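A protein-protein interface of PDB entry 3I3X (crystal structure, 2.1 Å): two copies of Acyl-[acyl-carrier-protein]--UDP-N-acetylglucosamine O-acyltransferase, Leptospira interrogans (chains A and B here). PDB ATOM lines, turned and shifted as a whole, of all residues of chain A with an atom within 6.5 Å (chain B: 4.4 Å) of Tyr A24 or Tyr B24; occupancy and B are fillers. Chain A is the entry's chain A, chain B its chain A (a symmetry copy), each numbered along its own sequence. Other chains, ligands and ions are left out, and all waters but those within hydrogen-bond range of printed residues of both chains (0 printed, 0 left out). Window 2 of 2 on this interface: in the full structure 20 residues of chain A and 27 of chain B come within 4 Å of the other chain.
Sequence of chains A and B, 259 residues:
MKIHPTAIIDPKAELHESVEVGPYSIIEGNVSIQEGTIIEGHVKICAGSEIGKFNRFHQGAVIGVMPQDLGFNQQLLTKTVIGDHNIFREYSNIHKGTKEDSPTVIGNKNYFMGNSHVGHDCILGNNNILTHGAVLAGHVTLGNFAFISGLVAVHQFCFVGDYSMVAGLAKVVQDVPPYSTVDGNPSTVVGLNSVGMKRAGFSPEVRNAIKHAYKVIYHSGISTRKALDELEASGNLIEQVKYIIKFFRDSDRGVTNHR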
ATOM      1  N   HIS A   4     -21.527  -0.175  12.154  1.00  0.00           N
ATOM      2  CA  HIS A   4     -22.409  -1.065  12.911  1.00  0.00           C
ATOM      3  C   HIS A   4     -23.028  -0.329  14.104  1.00  0.00           C
ATOM      4  O   HIS A   4     -22.334   0.441  14.777  1.00  0.00           O
ATOM      5  CB  HIS A   4     -21.659  -2.313  13.378  1.00  0.00           C
ATOM      6  CG  HIS A   4     -22.539  -3.512  13.562  1.00  0.00           C
ATOM      7  ND1 HIS A   4     -23.119  -3.834  14.772  1.00  0.00           N
ATOM      8  CD2 HIS A   4     -22.942  -4.465  12.687  1.00  0.00           C
ATOM      9  CE1 HIS A   4     -23.839  -4.932  14.633  1.00  0.00           C
ATOM     10  NE2 HIS A   4     -23.749  -5.336  13.378  1.00  0.00           N
ATOM     11  N   THR A   6     -23.961  -1.374  17.047  1.00  0.00           N
ATOM     12  CA  THR A   6     -23.463  -1.781  18.365  1.00  0.00           C
ATOM     13  C   THR A   6     -22.024  -1.330  18.647  1.00  0.00           C
ATOM     14  O   THR A   6     -21.363  -1.866  19.539  1.00  0.00           O
ATOM     15  CB  THR A   6     -23.578  -3.310  18.580  1.00  0.00           C
ATOM     16  OG1 THR A   6     -22.948  -4.002  17.494  1.00  0.00           O
ATOM     17  CG2 THR A   6     -25.033  -3.741  18.682  1.00  0.00           C
ATOM     18  N   ALA A   7     -21.545  -0.347  17.891  1.00  0.00           N
ATOM     19  CA  ALA A   7     -20.217   0.212  18.120  1.00  0.00           C
ATOM     20  C   ALA A   7     -20.296   1.443  19.028  1.00  0.00           C
ATOM     21  O   ALA A   7     -21.179   2.292  18.858  1.00  0.00           O
ATOM     22  CB  ALA A   7     -19.544   0.550  16.798  1.00  0.00           C
ATOM     23  N   ILE A   8     -19.384   1.520  19.999  1.00  0.00           N
ATOM     24  CA  ILE A   8     -19.301   2.666  20.900  1.00  0.00           C
ATOM     25  C   ILE A   8     -18.223   3.628  20.396  1.00  0.00           C
ATOM     26  O   ILE A   8     -17.028   3.440  20.661  1.00  0.00           O
ATOM     27  CB  ILE A   8     -18.989   2.252  22.369  1.00  0.00           C
ATOM     28  CG1 ILE A   8     -19.727   0.962  22.773  1.00  0.00           C
ATOM     29  CG2 ILE A   8     -19.244   3.423  23.338  1.00  0.00           C
ATOM     30  CD1 ILE A   8     -21.242   1.094  22.930  1.00  0.00           C
ATOM     31  N   GLY A  22     -16.798  -2.061  12.647  1.00  0.00           N
ATOM     32  CA  GLY A  22     -17.534  -3.316  12.830  1.00  0.00           C
ATOM     33  C   GLY A  22     -18.164  -3.462  14.202  1.00  0.00           C
ATOM     34  O   GLY A  22     -18.045  -2.559  15.034  1.00  0.00           O
ATOM     35  N   PRO A  23     -18.823  -4.616  14.460  1.00  0.00           N
ATOM     36  CA  PRO A  23     -19.584  -4.857  15.685  1.00  0.00           C
ATOM     37  C   PRO A  23     -18.749  -4.835  16.960  1.00  0.00           C
ATOM     38  O   PRO A  23     -17.665  -5.437  17.013  1.00  0.00           O
ATOM     39  CB  PRO A  23     -20.156  -6.264  15.480  1.00  0.00           C
ATOM     40  CG  PRO A  23     -20.047  -6.532  14.035  1.00  0.00           C
ATOM     41  CD  PRO A  23     -18.861  -5.784  13.564  1.00  0.00           C
ATOM     42  N   TYR A  24     -19.264  -4.137  17.974  1.00  0.00           N
ATOM     43  CA  TYR A  24     -18.725  -4.162  19.340  1.00  0.00           C
ATOM     44  C   TYR A  24     -17.321  -3.549  19.468  1.00  0.00           C
ATOM     45  O   TYR A  24     -16.611  -3.788  20.450  1.00  0.00           O
ATOM     46  CB  TYR A  24     -18.810  -5.584  19.940  1.00  0.00           C
ATOM     47  CG  TYR A  24     -20.165  -6.246  19.722  1.00  0.00           C
ATOM     48  CD1 TYR A  24     -20.300  -7.369  18.898  1.00  0.00           C
ATOM     49  CD2 TYR A  24     -21.316  -5.726  20.320  1.00  0.00           C
ATOM     50  CE1 TYR A  24     -21.547  -7.967  18.691  1.00  0.00           C
ATOM     51  CE2 TYR A  24     -22.563  -6.313  20.120  1.00  0.00           C
ATOM     52  CZ  TYR A  24     -22.674  -7.431  19.308  1.00  0.00           C
ATOM     53  OH  TYR A  24     -23.922  -7.997  19.118  1.00  0.00           O
ATOM     54  N   SER A  25     -16.941  -2.750  18.473  1.00  0.00           N
ATOM     55  CA  SER A  25     -15.721  -1.958  18.534  1.00  0.00           C
ATOM     56  C   SER A  25     -15.919  -0.717  19.410  1.00  0.00           C
ATOM     57  O   SER A  25     -17.046  -0.236  19.581  1.00  0.00           O
ATOM     58  CB  SER A  25     -15.267  -1.546  17.130  1.00  0.00           C
ATOM     59  OG  SER A  25     -14.849  -2.663  16.366  1.00  0.00           O
ATOM     60  N   ILE A  26     -14.818  -0.209  19.963  1.00  0.00           N
ATOM     61  CA  ILE A  26     -14.844   0.942  20.858  1.00  0.00           C
ATOM     62  C   ILE A  26     -13.824   1.996  20.415  1.00  0.00           C
ATOM     63  O   ILE A  26     -12.612   1.766  20.485  1.00  0.00           O
ATOM     64  CB  ILE A  26     -14.576   0.528  22.329  1.00  0.00           C
ATOM     65  CG1 ILE A  26     -15.538  -0.584  22.757  1.00  0.00           C
ATOM     66  CG2 ILE A  26     -14.692   1.743  23.260  1.00  0.00           C
ATOM     67  CD1 ILE A  26     -15.134  -1.338  23.991  1.00  0.00           C
ATOM     68  N   GLU A  40     -12.790  -3.771  11.789  1.00  0.00           N
ATOM     69  CA  GLU A  40     -13.654  -4.939  11.960  1.00  0.00           C
ATOM     70  C   GLU A  40     -14.356  -4.922  13.318  1.00  0.00           C
ATOM     71  O   GLU A  40     -14.729  -3.859  13.812  1.00  0.00           O
ATOM     72  CB  GLU A  40     -12.848  -6.230  11.801  1.00  0.00           C
ATOM     73  CG  GLU A  40     -12.253  -6.423  10.416  1.00  0.00           C
ATOM     74  CD  GLU A  40     -11.751  -7.836  10.189  1.00  0.00           C
ATOM     75  OE1 GLU A  40     -11.672  -8.604  11.170  1.00  0.00           O
ATOM     76  OE2 GLU A  40     -11.433  -8.177   9.031  1.00  0.00           O
ATOM     77  N   GLY A  41     -14.535  -6.096  13.918  1.00  0.00           N
ATOM     78  CA  GLY A  41     -15.203  -6.179  15.210  1.00  0.00           C
ATOM     79  C   GLY A  41     -14.244  -6.182  16.379  1.00  0.00           C
ATOM     80  O   GLY A  41     -13.062  -6.478  16.211  1.00  0.00           O
ATOM     81  N   HIS A  42     -14.755  -5.828  17.557  1.00  0.00           N
ATOM     82  CA  HIS A  42     -13.997  -5.830  18.821  1.00  0.00           C
ATOM     83  C   HIS A  42     -12.648  -5.095  18.775  1.00  0.00           C
ATOM     84  O   HIS A  42     -11.767  -5.369  19.586  1.00  0.00           O
ATOM     85  CB  HIS A  42     -13.804  -7.264  19.346  1.00  0.00           C
ATOM     86  CG  HIS A  42     -15.033  -8.112  19.253  1.00  0.00           C
ATOM     87  ND1 HIS A  42     -15.176  -9.111  18.314  1.00  0.00           N
ATOM     88  CD2 HIS A  42     -16.185  -8.099  19.967  1.00  0.00           C
ATOM     89  CE1 HIS A  42     -16.358  -9.685  18.461  1.00  0.00           C
ATOM     90  NE2 HIS A  42     -16.989  -9.091  19.457  1.00  0.00           N
ATOM     91  N   VAL A  43     -12.491  -4.177  17.827  1.00  0.00           N
ATOM     92  CA  VAL A  43     -11.309  -3.311  17.766  1.00  0.00           C
ATOM     93  C   VAL A  43     -11.452  -2.124  18.731  1.00  0.00           C
ATOM     94  O   VAL A  43     -12.523  -1.518  18.834  1.00  0.00           O
ATOM     95  CB  VAL A  43     -11.043  -2.803  16.312  1.00  0.00           C
ATOM     96  CG1 VAL A  43      -9.836  -1.872  16.254  1.00  0.00           C
ATOM     97  CG2 VAL A  43     -10.868  -3.977  15.342  1.00  0.00           C
ATOM     98  N   GLN A  59     -10.236  -8.046  13.677  1.00  0.00           N
ATOM     99  CA  GLN A  59     -10.873  -8.295  14.961  1.00  0.00           C
ATOM    100  C   GLN A  59      -9.958  -8.332  16.187  1.00  0.00           C
ATOM    101  O   GLN A  59      -8.993  -9.104  16.241  1.00  0.00           O
ATOM    102  CB  GLN A  59     -11.697  -9.585  14.912  1.00  0.00           C
ATOM    103  CG  GLN A  59     -11.865 -10.186  16.287  1.00  0.00           C
ATOM    104  CD  GLN A  59     -13.211 -10.813  16.534  1.00  0.00           C
ATOM    105  OE1 GLN A  59     -14.201 -10.487  15.866  1.00  0.00           O
ATOM    106  NE2 GLN A  59     -13.265 -11.710  17.533  1.00  0.00           N
ATOM    107  N   THR B   6     -27.420 -11.362  21.706  1.00  0.00           N
ATOM    108  CA  THR B   6     -26.460 -10.367  21.218  1.00  0.00           C
ATOM    109  C   THR B   6     -25.411 -10.941  20.258  1.00  0.00           C
ATOM    110  O   THR B   6     -24.365 -10.330  20.033  1.00  0.00           O
ATOM    111  CB  THR B   6     -25.750  -9.631  22.380  1.00  0.00           C
ATOM    112  OG1 THR B   6     -25.173 -10.585  23.280  1.00  0.00           O
ATOM    113  CG2 THR B   6     -26.721  -8.738  23.138  1.00  0.00           C
ATOM    114  N   ILE B   8     -24.259 -11.976  16.447  1.00  0.00           N
ATOM    115  CA  ILE B   8     -24.515 -11.651  15.046  1.00  0.00           C
ATOM    116  C   ILE B   8     -24.223 -12.878  14.181  1.00  0.00           C
ATOM    117  O   ILE B   8     -23.069 -13.143  13.820  1.00  0.00           O
ATOM    118  CB  ILE B   8     -23.665 -10.444  14.547  1.00  0.00           C
ATOM    119  CG1 ILE B   8     -23.540  -9.346  15.620  1.00  0.00           C
ATOM    120  CG2 ILE B   8     -24.197  -9.916  13.200  1.00  0.00           C
ATOM    121  CD1 ILE B   8     -24.822  -8.567  15.915  1.00  0.00           C
ATOM    122  N   GLY B  22     -22.291 -18.040  22.185  1.00  0.00           N
ATOM    123  CA  GLY B  22     -22.239 -17.137  23.338  1.00  0.00           C
ATOM    124  C   GLY B  22     -22.329 -15.667  22.970  1.00  0.00           C
ATOM    125  O   GLY B  22     -22.454 -15.335  21.789  1.00  0.00           O
ATOM    126  N   PRO B  23     -22.243 -14.771  23.982  1.00  0.00           N
ATOM    127  CA  PRO B  23     -22.435 -13.332  23.805  1.00  0.00           C
ATOM    128  C   PRO B  23     -21.416 -12.669  22.886  1.00  0.00           C
ATOM    129  O   PRO B  23     -20.206 -12.922  23.000  1.00  0.00           O
ATOM    130  CB  PRO B  23     -22.274 -12.774  25.223  1.00  0.00           C
ATOM    131  CG  PRO B  23     -22.433 -13.928  26.126  1.00  0.00           C
ATOM    132  CD  PRO B  23     -21.939 -15.107  25.382  1.00  0.00           C
ATOM    133  N   TYR B  24     -21.920 -11.828  21.981  1.00  0.00           N
ATOM    134  CA  TYR B  24     -21.100 -10.938  21.147  1.00  0.00           C
ATOM    135  C   TYR B  24     -20.200 -11.678  20.143  1.00  0.00           C
ATOM    136  O   TYR B  24     -19.234 -11.112  19.621  1.00  0.00           O
ATOM    137  CB  TYR B  24     -20.316  -9.933  22.021  1.00  0.00           C
ATOM    138  CG  TYR B  24     -21.174  -9.275  23.093  1.00  0.00           C
ATOM    139  CD1 TYR B  24     -20.953  -9.520  24.452  1.00  0.00           C
ATOM    140  CD2 TYR B  24     -22.228  -8.427  22.740  1.00  0.00           C
ATOM    141  CE1 TYR B  24     -21.750  -8.924  25.434  1.00  0.00           C
ATOM    142  CE2 TYR B  24     -23.029  -7.828  23.709  1.00  0.00           C
ATOM    143  CZ  TYR B  24     -22.787  -8.077  25.052  1.00  0.00           C
ATOM    144  OH  TYR B  24     -23.596  -7.476  25.998  1.00  0.00           O
ATOM    145  N   SER B  25     -20.537 -12.937  19.876  1.00  0.00           N
ATOM    146  CA  SER B  25     -19.896 -13.707  18.820  1.00  0.00           C
ATOM    147  C   SER B  25     -20.438 -13.304  17.445  1.00  0.00           C
ATOM    148  O   SER B  25     -21.566 -12.809  17.329  1.00  0.00           O
ATOM    149  CB  SER B  25     -20.090 -15.210  19.044  1.00  0.00           C
ATOM    150  OG  SER B  25     -19.396 -15.661  20.193  1.00  0.00           O
ATOM    151  N   ILE B  26     -19.628 -13.521  16.410  1.00  0.00           N
ATOM    152  CA  ILE B  26     -19.977 -13.151  15.042  1.00  0.00           C
ATOM    153  C   ILE B  26     -19.763 -14.331  14.091  1.00  0.00           C
ATOM    154  O   ILE B  26     -18.624 -14.752  13.856  1.00  0.00           O
ATOM    155  CB  ILE B  26     -19.164 -11.922  14.556  1.00  0.00           C
ATOM    156  CG1 ILE B  26     -19.306 -10.761  15.544  1.00  0.00           C
ATOM    157  CG2 ILE B  26     -19.611 -11.504  13.149  1.00  0.00           C
ATOM    158  CD1 ILE B  26     -18.276  -9.677  15.408  1.00  0.00           C
ATOM    159  N   HIS B  42     -17.454 -13.673  22.121  1.00  0.00           N
ATOM    160  CA  HIS B  42     -16.490 -12.975  21.250  1.00  0.00           C
ATOM    161  C   HIS B  42     -15.742 -13.873  20.253  1.00  0.00           C
ATOM    162  O   HIS B  42     -14.662 -13.515  19.789  1.00  0.00           O
ATOM    163  CB  HIS B  42     -15.489 -12.155  22.083  1.00  0.00           C
ATOM    164  CG  HIS B  42     -16.118 -11.389  23.202  1.00  0.00           C
ATOM    165  ND1 HIS B  42     -15.995 -11.767  24.523  1.00  0.00           N
ATOM    166  CD2 HIS B  42     -16.894 -10.277  23.202  1.00  0.00           C
ATOM    167  CE1 HIS B  42     -16.657 -10.915  25.287  1.00  0.00           C
ATOM    168  NE2 HIS B  42     -17.211 -10.002  24.511  1.00  0.00           N
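The backbone carbonyl oxygen (O) of Thr B6 sits at hydrogen-bond distance from the side-chain hydroxyl (OH) of Tyr A24, at 2.5 Å. The backbone carbonyl oxygen (O) of Tyr B24 is in hydrogen-bond range of a ring nitrogen (NE2) of His A42 (3.0 Å). O of His B42 lies within hydrogen-bond range of NE2 of Gln A59 (3.2 Å).
ND1 of His A4 lies within hydrogen-bond range of OG1 of Thr A6 (2.7 Å). N of Tyr A24 sits at hydrogen-bond distance from O of Thr A6. N of His A42 is in hydrogen-bond range of O of Pro A23 (3.0 Å). The backbone NH (N) of Gln A59 lies within hydrogen-bond range of the side-chain carboxylate (OE1) of Glu A40 (2.9 Å). O of Pro B23 sits at hydrogen-bond distance from N of His B42 (3.0 Å). The backbone NH (N) of His B42 lies within hydrogen-bond range of the side-chain hydroxyl (OG) of Ser B25, at 3.4 Å.
Among the printed residues, merely in contact across the chains: Tyr A24 with Ile B8 (3.4 Å), Tyr A24 with Tyr B24 (3.4 Å), His A42 with Ile B26 (3.6 Å), Pro A23 with Ile B26 (3.9 Å), His A42 with His B42 (3.9 Å) and His A4 with Ile B8 (3.98 Å).
Of chain B, only Thr B6 (2.5 Å), Ile B8 (3.4 Å) and Tyr B24 (3.4 Å) come within 4 Å of Tyr A24. Tyr B24 touches two residues of chain A. Of the printed residues of chain A, Thr B6 touches Tyr A24. Of the printed residues of chain B, His A42 touches Tyr B24 (3.0 Å), Ile B26 (3.6 Å) and His B42 (3.9 Å). Pro B23 touches none of the printed residues of chain A. The nearest printed residue of chain A that does not touch Ile B26 is Gln A59 (4.2 Å).
Of the 14 printed residues of chain A, 5 touch a printed residue of chain B. Printed residues of chain A that touch a printed residue of chain B: His A4, Pro A23, Tyr A24, His A42 and Gln A59. Of the 8 printed residues of chain B, 5 touch a printed residue of chain A.
Tyr A24 touches Thr B6, but with the chains exchanged Thr A6 does not touch Tyr B24 (6.7 Å). Tyr A24 touches Ile B8, but with the chains exchanged Ile A8 does not touch Tyr B24 (9.1 Å). Tyr A24 touches its own counterpart, Tyr B24. His A42 touches Tyr B24, but with the chains exchanged Tyr A24 does not touch His B42 (6.0 Å). Of the 9 pairs that touch across the chains among the printed residues, 2 have their exchanged pair printed and touching as well.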
